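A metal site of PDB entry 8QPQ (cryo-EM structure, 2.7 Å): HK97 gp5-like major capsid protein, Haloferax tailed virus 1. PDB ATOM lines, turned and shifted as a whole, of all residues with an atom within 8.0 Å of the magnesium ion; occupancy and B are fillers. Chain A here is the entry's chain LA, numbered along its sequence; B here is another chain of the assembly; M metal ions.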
ATOM      1  N   ASP A 259      25.264  11.353 -18.063  1.00  0.00           N
ATOM      2  CA  ASP A 259      25.646  11.205 -16.665  1.00  0.00           C
ATOM      3  C   ASP A 259      26.363  12.444 -16.118  1.00  0.00           C
ATOM      4  O   ASP A 259      26.639  12.531 -14.931  1.00  0.00           O
ATOM      5  CB  ASP A 259      26.488   9.946 -16.462  1.00  0.00           C
ATOM      6  CG  ASP A 259      27.766   9.900 -17.277  1.00  0.00           C
ATOM      7  OD1 ASP A 259      28.214  10.962 -17.795  1.00  0.00           O
ATOM      8  OD2 ASP A 259      28.316   8.760 -17.422  1.00  0.00           O
ATOM      9  N   PRO A 296      25.146  18.713  -2.559  1.00  0.00           N
ATOM     10  CA  PRO A 296      25.136  17.395  -3.166  1.00  0.00           C
ATOM     11  C   PRO A 296      24.128  17.239  -4.306  1.00  0.00           C
ATOM     12  O   PRO A 296      24.420  16.535  -5.265  1.00  0.00           O
ATOM     13  CB  PRO A 296      24.860  16.439  -1.989  1.00  0.00           C
ATOM     14  CG  PRO A 296      24.192  17.294  -0.936  1.00  0.00           C
ATOM     15  CD  PRO A 296      24.832  18.644  -1.122  1.00  0.00           C
ATOM     16  N   ILE A 297      22.979  17.933  -4.241  1.00  0.00           N
ATOM     17  CA  ILE A 297      21.938  17.873  -5.273  1.00  0.00           C
ATOM     18  C   ILE A 297      22.434  18.384  -6.620  1.00  0.00           C
ATOM     19  O   ILE A 297      22.001  17.911  -7.669  1.00  0.00           O
ATOM     20  CB  ILE A 297      20.668  18.667  -4.862  1.00  0.00           C
ATOM     21  CG1 ILE A 297      20.209  18.417  -3.435  1.00  0.00           C
ATOM     22  CG2 ILE A 297      19.560  18.533  -5.888  1.00  0.00           C
ATOM     23  CD1 ILE A 297      19.730  17.031  -3.191  1.00  0.00           C
ATOM     24  N   GLY A 299      25.380  18.016  -7.986  1.00  0.00           N
ATOM     25  CA  GLY A 299      26.026  16.884  -8.650  1.00  0.00           C
ATOM     26  C   GLY A 299      25.161  15.618  -8.736  1.00  0.00           C
ATOM     27  O   GLY A 299      25.662  14.547  -9.043  1.00  0.00           O
ATOM     28  N   ASP A 300      23.845  15.729  -8.467  1.00  0.00           N
ATOM     29  CA  ASP A 300      22.934  14.603  -8.397  1.00  0.00           C
ATOM     30  C   ASP A 300      21.541  15.061  -8.855  1.00  0.00           C
ATOM     31  O   ASP A 300      20.612  15.080  -8.034  1.00  0.00           O
ATOM     32  CB  ASP A 300      22.950  13.971  -6.994  1.00  0.00           C
ATOM     33  CG  ASP A 300      22.270  12.619  -6.860  1.00  0.00           C
ATOM     34  OD1 ASP A 300      22.230  11.870  -7.872  1.00  0.00           O
ATOM     35  OD2 ASP A 300      21.804  12.312  -5.734  1.00  0.00           O
ATOM     36  N   ILE A 301      21.433  15.474 -10.114  1.00  0.00           N
ATOM     37  CA  ILE A 301      20.181  16.048 -10.645  1.00  0.00           C
ATOM     38  C   ILE A 301      19.870  15.485 -12.017  1.00  0.00           C
ATOM     39  O   ILE A 301      20.775  15.221 -12.806  1.00  0.00           O
ATOM     40  CB  ILE A 301      20.262  17.590 -10.687  1.00  0.00           C
ATOM     41  CG1 ILE A 301      18.942  18.225 -11.120  1.00  0.00           C
ATOM     42  CG2 ILE A 301      21.418  18.096 -11.551  1.00  0.00           C
ATOM     43  CD1 ILE A 301      18.886  19.724 -10.875  1.00  0.00           C
ATOM     44  N   ALA A 302      18.577  15.197 -12.273  1.00  0.00           N
ATOM     45  CA  ALA A 302      18.075  14.678 -13.544  1.00  0.00           C
ATOM     46  C   ALA A 302      18.776  13.388 -14.011  1.00  0.00           C
ATOM     47  O   ALA A 302      18.867  13.118 -15.211  1.00  0.00           O
ATOM     48  CB  ALA A 302      18.074  15.772 -14.612  1.00  0.00           C
ATOM     49  N   GLY A 303      19.244  12.563 -13.058  1.00  0.00           N
ATOM     50  CA  GLY A 303      19.923  11.316 -13.367  1.00  0.00           C
ATOM     51  C   GLY A 303      21.421  11.481 -13.668  1.00  0.00           C
ATOM     52  O   GLY A 303      22.108  10.503 -13.949  1.00  0.00           O
ATOM     53  N   LEU A 304      21.943  12.706 -13.548  1.00  0.00           N
ATOM     54  CA  LEU A 304      23.342  13.032 -13.788  1.00  0.00           C
ATOM     55  C   LEU A 304      24.089  12.969 -12.456  1.00  0.00           C
ATOM     56  O   LEU A 304      23.582  13.480 -11.428  1.00  0.00           O
ATOM     57  CB  LEU A 304      23.446  14.422 -14.431  1.00  0.00           C
ATOM     58  CG  LEU A 304      22.507  14.682 -15.612  1.00  0.00           C
ATOM     59  CD1 LEU A 304      22.613  16.114 -16.053  1.00  0.00           C
ATOM     60  CD2 LEU A 304      22.881  13.785 -16.754  1.00  0.00           C
ATOM     61  N   ASP A 305      25.258  12.324 -12.474  1.00  0.00           N
ATOM     62  CA  ASP A 305      26.057  12.088 -11.272  1.00  0.00           C
ATOM     63  C   ASP A 305      27.291  12.977 -11.194  1.00  0.00           C
ATOM     64  O   ASP A 305      28.081  12.837 -10.243  1.00  0.00           O
ATOM     65  CB  ASP A 305      26.304  10.566 -11.106  1.00  0.00           C
ATOM     66  CG  ASP A 305      25.032   9.826 -10.696  1.00  0.00           C
ATOM     67  OD1 ASP A 305      24.234  10.408  -9.897  1.00  0.00           O
ATOM     68  OD2 ASP A 305      24.878   8.616 -11.082  1.00  0.00           O
ATOM     69  N   MET A 306      27.502  13.866 -12.166  1.00  0.00           N
ATOM     70  CA  MET A 306      28.618  14.802 -12.106  1.00  0.00           C
ATOM     71  C   MET A 306      28.204  16.187 -12.631  1.00  0.00           C
ATOM     72  O   MET A 306      27.586  16.317 -13.687  1.00  0.00           O
ATOM     73  CB  MET A 306      29.820  14.281 -12.883  1.00  0.00           C
ATOM     74  CG  MET A 306      30.999  15.218 -12.832  1.00  0.00           C
ATOM     75  SD  MET A 306      32.489  14.620 -13.685  1.00  0.00           S
ATOM     76  CE  MET A 306      32.917  13.167 -12.723  1.00  0.00           C
ATOM     77  N   GLU B 287      13.695  12.021  -5.146  1.00  0.00           N
ATOM     78  CA  GLU B 287      14.289  11.011  -6.009  1.00  0.00           C
ATOM     79  C   GLU B 287      14.105  11.253  -7.509  1.00  0.00           C
ATOM     80  O   GLU B 287      15.014  10.969  -8.273  1.00  0.00           O
ATOM     81  CB  GLU B 287      13.796   9.633  -5.598  1.00  0.00           C
ATOM     82  CG  GLU B 287      14.475   9.080  -4.368  1.00  0.00           C
ATOM     83  CD  GLU B 287      15.872   8.513  -4.581  1.00  0.00           C
ATOM     84  OE1 GLU B 287      16.512   8.743  -5.633  1.00  0.00           O
ATOM     85  OE2 GLU B 287      16.314   7.817  -3.672  1.00  0.00           O
ATOM     86  N   LEU B 289      13.682  14.297  -9.003  1.00  0.00           N
ATOM     87  CA  LEU B 289      14.533  15.451  -9.262  1.00  0.00           C
ATOM     88  C   LEU B 289      16.005  15.034  -9.327  1.00  0.00           C
ATOM     89  O   LEU B 289      16.724  15.487 -10.228  1.00  0.00           O
ATOM     90  CB  LEU B 289      14.267  16.490  -8.165  1.00  0.00           C
ATOM     91  CG  LEU B 289      15.127  17.750  -8.259  1.00  0.00           C
ATOM     92  CD1 LEU B 289      14.317  19.008  -8.020  1.00  0.00           C
ATOM     93  CD2 LEU B 289      16.271  17.708  -7.267  1.00  0.00           C
ATOM     94  N   ARG B 290      16.427  14.139  -8.452  1.00  0.00           N
ATOM     95  CA  ARG B 290      17.813  13.676  -8.369  1.00  0.00           C
ATOM     96  C   ARG B 290      18.146  12.628  -9.428  1.00  0.00           C
ATOM     97  O   ARG B 290      19.051  12.829 -10.228  1.00  0.00           O
ATOM     98  CB  ARG B 290      18.140  13.155  -6.959  1.00  0.00           C
ATOM     99  CG  ARG B 290      18.141  14.217  -5.892  1.00  0.00           C
ATOM    100  CD  ARG B 290      18.827  13.753  -4.630  1.00  0.00           C
ATOM    101  NE  ARG B 290      18.138  12.675  -3.927  1.00  0.00           N
ATOM    102  CZ  ARG B 290      18.613  11.437  -3.786  1.00  0.00           C
ATOM    103  NH1 ARG B 290      17.954  10.567  -3.049  1.00  0.00           N
ATOM    104  NH2 ARG B 290      19.813  11.097  -4.235  1.00  0.00           N
ATOM    105  N   ASN B 291      17.430  11.497  -9.443  1.00  0.00           N
ATOM    106  CA  ASN B 291      17.803  10.279 -10.145  1.00  0.00           C
ATOM    107  C   ASN B 291      16.894   9.948 -11.327  1.00  0.00           C
ATOM    108  O   ASN B 291      17.138   8.956 -12.010  1.00  0.00           O
ATOM    109  CB  ASN B 291      17.972   9.119  -9.138  1.00  0.00           C
ATOM    110  CG  ASN B 291      19.145   9.355  -8.225  1.00  0.00           C
ATOM    111  OD1 ASN B 291      20.238   9.578  -8.693  1.00  0.00           O
ATOM    112  ND2 ASN B 291      18.931   9.357  -6.907  1.00  0.00           N
ATOM    113  N   ARG B 292      15.868  10.753 -11.584  1.00  0.00           N
ATOM    114  CA  ARG B 292      15.020  10.710 -12.784  1.00  0.00           C
ATOM    115  C   ARG B 292      14.323   9.357 -12.938  1.00  0.00           C
ATOM    116  O   ARG B 292      13.534   9.023 -12.034  1.00  0.00           O
ATOM    117  CB  ARG B 292      15.786  11.190 -14.018  1.00  0.00           C
ATOM    118  CG  ARG B 292      14.856  11.911 -14.981  1.00  0.00           C
ATOM    119  CD  ARG B 292      15.530  12.396 -16.257  1.00  0.00           C
ATOM    120  NE  ARG B 292      15.482  11.273 -17.170  1.00  0.00           N
ATOM    121  CZ  ARG B 292      14.953  11.254 -18.387  1.00  0.00           C
ATOM    122  NH1 ARG B 292      14.991  10.110 -19.061  1.00  0.00           N
ATOM    123  NH2 ARG B 292      14.424  12.334 -18.936  1.00  0.00           N
ATOM    124  N   ASP B 294      15.519   6.378 -12.581  1.00  0.00           N
ATOM    125  CA  ASP B 294      16.071   5.445 -11.599  1.00  0.00           C
ATOM    126  C   ASP B 294      15.445   5.620 -10.203  1.00  0.00           C
ATOM    127  O   ASP B 294      15.755   4.840  -9.302  1.00  0.00           O
ATOM    128  CB  ASP B 294      17.597   5.545 -11.542  1.00  0.00           C
ATOM    129  CG  ASP B 294      18.331   5.328 -12.851  1.00  0.00           C
ATOM    130  OD1 ASP B 294      17.810   4.617 -13.731  1.00  0.00           O
ATOM    131  OD2 ASP B 294      19.485   5.745 -12.912  1.00  0.00           O
HETATM  132 MG    MG M   1      22.103  10.257  -9.075  1.00  0.00          MG
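ND2 of Asn 291 of chain B sits close to NH2 of Arg 290 of chain B (3.3 Å).
ND2 of Asn 291 of chain B is in hydrogen-bond range of OE1 of Glu 287 of chain B, at 2.8 Å.
The backbone NH of Asp 305 sits at hydrogen-bond distance from the backbone carbonyl oxygen of Asp 259, at 2.8 Å.
NH2 of Arg 290 of chain B lies within salt-bridge range of OD2 of Asp 300 (2.8 Å).
Three residues have an atom within 4 Å of the magnesium ion: Asp 300, Asp 305 and Asn 291 of chain B.
The nearest printed residue that does not touch the magnesium ion is Arg 290 of chain B (4.2 Å).
The side-chain carboxylate (OD1) of Asp 300 binds the magnesium ion, 2.0 Å away.
OD1 of Asn 291 of chain B binds the magnesium ion (2.0 Å).
The magnesium ion is bound by OD1 of Asp 305 (2.3 Å).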
